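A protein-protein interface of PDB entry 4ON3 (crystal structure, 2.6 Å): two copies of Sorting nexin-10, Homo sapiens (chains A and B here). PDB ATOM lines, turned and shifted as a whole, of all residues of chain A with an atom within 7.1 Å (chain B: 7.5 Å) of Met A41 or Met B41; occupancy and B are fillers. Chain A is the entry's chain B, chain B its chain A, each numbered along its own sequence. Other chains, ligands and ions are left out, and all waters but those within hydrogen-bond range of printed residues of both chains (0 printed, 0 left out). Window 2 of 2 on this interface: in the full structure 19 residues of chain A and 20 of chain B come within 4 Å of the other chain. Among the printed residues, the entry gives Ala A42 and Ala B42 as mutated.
OE1 of Glu B9 lies within hydrogen-bond range of N of Met B41 (3.3 Å). O of Lys B46 lies within hydrogen-bond range of N of Thr B38, 3.1 Å away. The backbone carbonyl oxygen (O) of Ser B40 lies within hydrogen-bond range of the side-chain amino group (NZ) of Lys B46 (3.0 Å). N of Thr A38 sits at hydrogen-bond distance from O of Lys A46, 3.0 Å away. The backbone carbonyl oxygen of Ser A40 lies within hydrogen-bond range of the side-chain amino group of Lys A46 (3.2 Å). O of Phe A43 is in hydrogen-bond range of NZ of Lys A46, at 3.4 Å.
Met A41 touches its own counterpart, Met B41. Thr A44 touches Lys B46, and with the chains exchanged Lys A46 touches Thr B44. 10 positions are printed for both chains. Of the 3 pairs that touch across the chains among the printed residues, 3 have their exchanged pair printed and touching as well.
Ser A40 touches none of the printed residues of chain B. Printed residues of chain B within 4 Å of Met A41: Met B41 (3.96 Å). Printed residues of chain B within 4 Å of Thr A44: Lys B46. Printed residues of chain B within 4 Å of Lys A46: Thr B44 (3.4 Å). Met B41 touches just one residue of chain A: Met A41 (3.96 Å). Printed residues of chain A within 4 Å of Thr B44: Lys A46 (3.4 Å). Of the printed residues of chain A, Lys B46 touches Thr A44 (3.3 Å).
SD of Met B41 touches SD of Met A41 (3.96 Å). O of Thr A44 touches CG of Lys B46, at 3.3 Å. Lys A46 touches Thr B44 (CG to O, 3.4 Å).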
ATOM      1  N   GLU A   9     -10.780   1.377  -3.568  1.00  0.00           N
ATOM      2  CA  GLU A   9     -10.495  -0.030  -3.211  1.00  0.00           C
ATOM      3  C   GLU A   9     -10.717  -1.114  -4.259  1.00  0.00           C
ATOM      4  O   GLU A   9     -11.807  -1.246  -4.795  1.00  0.00           O
ATOM      5  CB  GLU A   9     -11.363  -0.464  -2.050  1.00  0.00           C
ATOM      6  CG  GLU A   9     -11.037   0.142  -0.709  1.00  0.00           C
ATOM      7  CD  GLU A   9     -11.969  -0.438   0.341  1.00  0.00           C
ATOM      8  OE1 GLU A   9     -12.776   0.329   0.925  1.00  0.00           O
ATOM      9  OE2 GLU A   9     -11.922  -1.677   0.536  1.00  0.00           O
ATOM     10  N   THR A  38      -4.449  -6.424  -3.387  1.00  0.00           N
ATOM     11  CA  THR A  38      -5.487  -5.524  -2.912  1.00  0.00           C
ATOM     12  C   THR A  38      -4.844  -4.304  -2.263  1.00  0.00           C
ATOM     13  O   THR A  38      -3.662  -4.324  -1.899  1.00  0.00           O
ATOM     14  CB  THR A  38      -6.378  -6.268  -1.900  1.00  0.00           C
ATOM     15  OG1 THR A  38      -7.504  -5.472  -1.557  1.00  0.00           O
ATOM     16  CG2 THR A  38      -5.603  -6.603  -0.635  1.00  0.00           C
ATOM     17  N   ASN A  39      -5.647  -3.258  -2.129  1.00  0.00           N
ATOM     18  CA  ASN A  39      -5.302  -2.103  -1.304  1.00  0.00           C
ATOM     19  C   ASN A  39      -6.306  -1.920  -0.139  1.00  0.00           C
ATOM     20  O   ASN A  39      -6.277  -0.901   0.575  1.00  0.00           O
ATOM     21  CB  ASN A  39      -5.320  -0.854  -2.166  1.00  0.00           C
ATOM     22  CG  ASN A  39      -6.687  -0.606  -2.692  1.00  0.00           C
ATOM     23  OD1 ASN A  39      -7.635  -1.116  -2.111  1.00  0.00           O
ATOM     24  ND2 ASN A  39      -6.818   0.115  -3.794  1.00  0.00           N
ATOM     25  N   SER A  40      -7.186  -2.891   0.065  1.00  0.00           N
ATOM     26  CA  SER A  40      -8.202  -2.735   1.065  1.00  0.00           C
ATOM     27  C   SER A  40      -7.643  -2.941   2.473  1.00  0.00           C
ATOM     28  O   SER A  40      -6.659  -3.642   2.675  1.00  0.00           O
ATOM     29  CB  SER A  40      -9.395  -3.663   0.782  1.00  0.00           C
ATOM     30  OG  SER A  40      -9.806  -4.320   1.973  1.00  0.00           O
ATOM     31  N   MET A  41      -8.327  -2.317   3.422  1.00  0.00           N
ATOM     32  CA  MET A  41      -7.996  -2.326   4.844  1.00  0.00           C
ATOM     33  C   MET A  41      -8.388  -3.645   5.460  1.00  0.00           C
ATOM     34  O   MET A  41      -7.765  -4.087   6.459  1.00  0.00           O
ATOM     35  CB  MET A  41      -8.702  -1.137   5.602  1.00  0.00           C
ATOM     36  CG  MET A  41      -8.122   0.278   5.352  1.00  0.00           C
ATOM     37  SD  MET A  41      -6.309   0.430   5.638  1.00  0.00           S
ATOM     38  CE  MET A  41      -5.489   0.044   4.054  1.00  0.00           C
ATOM     39  N   ALA A  42      -9.412  -4.243   4.844  1.00  0.00           N
ATOM     40  CA  ALA A  42      -9.878  -5.613   5.126  1.00  0.00           C
ATOM     41  C   ALA A  42      -8.777  -6.676   5.156  1.00  0.00           C
ATOM     42  O   ALA A  42      -8.833  -7.584   5.986  1.00  0.00           O
ATOM     43  CB  ALA A  42     -10.934  -6.036   4.125  1.00  0.00           C
ATOM     44  N   PHE A  43      -7.794  -6.552   4.266  1.00  0.00           N
ATOM     45  CA  PHE A  43      -6.655  -7.446   4.273  1.00  0.00           C
ATOM     46  C   PHE A  43      -5.448  -6.919   5.000  1.00  0.00           C
ATOM     47  O   PHE A  43      -5.124  -5.748   4.905  1.00  0.00           O
ATOM     48  CB  PHE A  43      -6.244  -7.788   2.842  1.00  0.00           C
ATOM     49  CG  PHE A  43      -7.195  -8.713   2.173  1.00  0.00           C
ATOM     50  CD1 PHE A  43      -8.330  -8.219   1.554  1.00  0.00           C
ATOM     51  CD2 PHE A  43      -6.992 -10.077   2.232  1.00  0.00           C
ATOM     52  CE1 PHE A  43      -9.233  -9.070   0.975  1.00  0.00           C
ATOM     53  CE2 PHE A  43      -7.895 -10.948   1.659  1.00  0.00           C
ATOM     54  CZ  PHE A  43      -9.013 -10.443   1.025  1.00  0.00           C
ATOM     55  N   THR A  44      -4.758  -7.825   5.673  1.00  0.00           N
ATOM     56  CA  THR A  44      -3.538  -7.520   6.372  1.00  0.00           C
ATOM     57  C   THR A  44      -2.398  -7.286   5.380  1.00  0.00           C
ATOM     58  O   THR A  44      -1.654  -6.315   5.489  1.00  0.00           O
ATOM     59  CB  THR A  44      -3.126  -8.670   7.327  1.00  0.00           C
ATOM     60  OG1 THR A  44      -4.062  -8.801   8.391  1.00  0.00           O
ATOM     61  CG2 THR A  44      -1.758  -8.439   7.962  1.00  0.00           C
ATOM     62  N   LYS A  46      -1.010  -6.780   1.503  1.00  0.00           N
ATOM     63  CA  LYS A  46      -1.564  -6.192   0.280  1.00  0.00           C
ATOM     64  C   LYS A  46      -1.293  -7.115  -0.920  1.00  0.00           C
ATOM     65  O   LYS A  46      -1.911  -6.961  -1.964  1.00  0.00           O
ATOM     66  CB  LYS A  46      -1.013  -4.784   0.064  1.00  0.00           C
ATOM     67  CG  LYS A  46      -1.221  -3.874   1.260  1.00  0.00           C
ATOM     68  CD  LYS A  46      -2.371  -2.886   1.101  1.00  0.00           C
ATOM     69  CE  LYS A  46      -2.732  -2.276   2.452  1.00  0.00           C
ATOM     70  NZ  LYS A  46      -3.549  -3.308   3.187  1.00  0.00           N
ATOM     71  N   HIS A 118      -8.952 -15.285   5.921  1.00  0.00           N
ATOM     72  CA  HIS A 118      -7.684 -14.603   5.870  1.00  0.00           C
ATOM     73  C   HIS A 118      -6.528 -15.485   6.120  1.00  0.00           C
ATOM     74  O   HIS A 118      -5.561 -15.352   5.450  1.00  0.00           O
ATOM     75  CB  HIS A 118      -7.708 -13.444   6.848  1.00  0.00           C
ATOM     76  CG  HIS A 118      -8.622 -12.357   6.387  1.00  0.00           C
ATOM     77  ND1 HIS A 118      -8.208 -11.343   5.533  1.00  0.00           N
ATOM     78  CD2 HIS A 118      -9.952 -12.201   6.544  1.00  0.00           C
ATOM     79  CE1 HIS A 118      -9.237 -10.600   5.207  1.00  0.00           C
ATOM     80  NE2 HIS A 118     -10.304 -11.098   5.810  1.00  0.00           N
ATOM     81  N   GLU B   9       0.922  -1.391  17.877  1.00  0.00           N
ATOM     82  CA  GLU B   9       1.766  -0.975  16.694  1.00  0.00           C
ATOM     83  C   GLU B   9       3.240  -1.034  16.880  1.00  0.00           C
ATOM     84  O   GLU B   9       3.720  -0.713  17.938  1.00  0.00           O
ATOM     85  CB  GLU B   9       1.392   0.404  16.149  1.00  0.00           C
ATOM     86  CG  GLU B   9      -0.007   0.364  15.521  1.00  0.00           C
ATOM     87  CD  GLU B   9      -0.308   1.498  14.528  1.00  0.00           C
ATOM     88  OE1 GLU B   9      -1.279   1.335  13.691  1.00  0.00           O
ATOM     89  OE2 GLU B   9       0.422   2.543  14.587  1.00  0.00           O
ATOM     90  N   PHE B  10       3.949  -1.520  15.857  1.00  0.00           N
ATOM     91  CA  PHE B  10       5.426  -1.628  15.882  1.00  0.00           C
ATOM     92  C   PHE B  10       5.948  -1.340  14.485  1.00  0.00           C
ATOM     93  O   PHE B  10       5.238  -1.563  13.483  1.00  0.00           O
ATOM     94  CB  PHE B  10       5.933  -3.016  16.333  1.00  0.00           C
ATOM     95  CG  PHE B  10       5.712  -4.088  15.319  1.00  0.00           C
ATOM     96  CD1 PHE B  10       4.507  -4.786  15.272  1.00  0.00           C
ATOM     97  CD2 PHE B  10       6.666  -4.365  14.353  1.00  0.00           C
ATOM     98  CE1 PHE B  10       4.278  -5.749  14.298  1.00  0.00           C
ATOM     99  CE2 PHE B  10       6.446  -5.356  13.393  1.00  0.00           C
ATOM    100  CZ  PHE B  10       5.253  -6.035  13.358  1.00  0.00           C
ATOM    101  N   THR B  38       6.459  -3.997   9.724  1.00  0.00           N
ATOM    102  CA  THR B  38       5.623  -3.187  10.525  1.00  0.00           C
ATOM    103  C   THR B  38       4.194  -3.657  10.408  1.00  0.00           C
ATOM    104  O   THR B  38       3.825  -4.321   9.432  1.00  0.00           O
ATOM    105  CB  THR B  38       5.648  -1.728  10.058  1.00  0.00           C
ATOM    106  OG1 THR B  38       4.871  -0.900  10.960  1.00  0.00           O
ATOM    107  CG2 THR B  38       5.078  -1.592   8.613  1.00  0.00           C
ATOM    108  N   ASN B  39       3.382  -3.284  11.401  1.00  0.00           N
ATOM    109  CA  ASN B  39       1.946  -3.532  11.347  1.00  0.00           C
ATOM    110  C   ASN B  39       1.168  -2.258  11.409  1.00  0.00           C
ATOM    111  O   ASN B  39      -0.055  -2.281  11.517  1.00  0.00           O
ATOM    112  CB  ASN B  39       1.528  -4.428  12.501  1.00  0.00           C
ATOM    113  CG  ASN B  39       1.624  -3.741  13.812  1.00  0.00           C
ATOM    114  OD1 ASN B  39       1.839  -2.535  13.876  1.00  0.00           O
ATOM    115  ND2 ASN B  39       1.529  -4.495  14.865  1.00  0.00           N
ATOM    116  N   SER B  40       1.897  -1.152  11.317  1.00  0.00           N
ATOM    117  CA  SER B  40       1.314   0.176  11.390  1.00  0.00           C
ATOM    118  C   SER B  40       0.449   0.599  10.214  1.00  0.00           C
ATOM    119  O   SER B  40       0.817   0.374   9.090  1.00  0.00           O
ATOM    120  CB  SER B  40       2.433   1.177  11.478  1.00  0.00           C
ATOM    121  OG  SER B  40       1.922   2.460  11.261  1.00  0.00           O
ATOM    122  N   MET B  41      -0.655   1.283  10.488  1.00  0.00           N
ATOM    123  CA  MET B  41      -1.496   1.862   9.440  1.00  0.00           C
ATOM    124  C   MET B  41      -0.731   2.925   8.634  1.00  0.00           C
ATOM    125  O   MET B  41      -1.160   3.323   7.557  1.00  0.00           O
ATOM    126  CB  MET B  41      -2.794   2.463  10.038  1.00  0.00           C
ATOM    127  CG  MET B  41      -3.964   1.488  10.317  1.00  0.00           C
ATOM    128  SD  MET B  41      -4.315   0.189   9.056  1.00  0.00           S
ATOM    129  CE  MET B  41      -3.236  -1.162   9.539  1.00  0.00           C
ATOM    130  N   ALA B  42       0.408   3.364   9.169  1.00  0.00           N
ATOM    131  CA  ALA B  42       1.266   4.415   8.570  1.00  0.00           C
ATOM    132  C   ALA B  42       1.918   4.000   7.230  1.00  0.00           C
ATOM    133  O   ALA B  42       2.104   4.847   6.343  1.00  0.00           O
ATOM    134  CB  ALA B  42       2.358   4.852   9.558  1.00  0.00           C
ATOM    135  N   PHE B  43       2.232   2.709   7.107  1.00  0.00           N
ATOM    136  CA  PHE B  43       2.793   2.148   5.910  1.00  0.00           C
ATOM    137  C   PHE B  43       1.775   1.551   4.985  1.00  0.00           C
ATOM    138  O   PHE B  43       0.778   1.076   5.423  1.00  0.00           O
ATOM    139  CB  PHE B  43       3.801   1.128   6.313  1.00  0.00           C
ATOM    140  CG  PHE B  43       5.034   1.751   6.824  1.00  0.00           C
ATOM    141  CD1 PHE B  43       5.130   2.135   8.155  1.00  0.00           C
ATOM    142  CD2 PHE B  43       6.085   2.049   5.957  1.00  0.00           C
ATOM    143  CE1 PHE B  43       6.297   2.724   8.614  1.00  0.00           C
ATOM    144  CE2 PHE B  43       7.237   2.649   6.412  1.00  0.00           C
ATOM    145  CZ  PHE B  43       7.336   2.984   7.725  1.00  0.00           C
ATOM    146  N   THR B  44       2.046   1.567   3.697  1.00  0.00           N
ATOM    147  CA  THR B  44       1.249   0.861   2.742  1.00  0.00           C
ATOM    148  C   THR B  44       1.560  -0.640   2.769  1.00  0.00           C
ATOM    149  O   THR B  44       0.635  -1.452   2.785  1.00  0.00           O
ATOM    150  CB  THR B  44       1.465   1.392   1.330  1.00  0.00           C
ATOM    151  OG1 THR B  44       1.279   2.816   1.311  1.00  0.00           O
ATOM    152  CG2 THR B  44       0.440   0.769   0.365  1.00  0.00           C
ATOM    153  N   LYS B  46       3.412  -3.952   4.606  1.00  0.00           N
ATOM    154  CA  LYS B  46       3.785  -4.314   5.965  1.00  0.00           C
ATOM    155  C   LYS B  46       5.139  -4.910   5.930  1.00  0.00           C
ATOM    156  O   LYS B  46       5.751  -5.081   6.940  1.00  0.00           O
ATOM    157  CB  LYS B  46       2.788  -5.288   6.595  1.00  0.00           C
ATOM    158  CG  LYS B  46       1.289  -5.069   6.299  1.00  0.00           C
ATOM    159  CD  LYS B  46       0.560  -4.049   7.162  1.00  0.00           C
ATOM    160  CE  LYS B  46       0.987  -2.634   6.788  1.00  0.00           C
ATOM    161  NZ  LYS B  46      -0.094  -1.613   7.041  1.00  0.00           N
ATOM    162  N   HIS B 118       8.451   7.281   2.437  1.00  0.00           N
ATOM    163  CA  HIS B 118       7.749   6.063   2.087  1.00  0.00           C
ATOM    164  C   HIS B 118       8.193   5.480   0.772  1.00  0.00           C
ATOM    165  O   HIS B 118       8.562   4.290   0.706  1.00  0.00           O
ATOM    166  CB  HIS B 118       6.271   6.286   2.200  1.00  0.00           C
ATOM    167  CG  HIS B 118       5.818   6.341   3.637  1.00  0.00           C
ATOM    168  ND1 HIS B 118       5.699   5.217   4.431  1.00  0.00           N
ATOM    169  CD2 HIS B 118       5.514   7.387   4.437  1.00  0.00           C
ATOM    170  CE1 HIS B 118       5.341   5.567   5.649  1.00  0.00           C
ATOM    171  NE2 HIS B 118       5.225   6.880   5.679  1.00  0.00           N
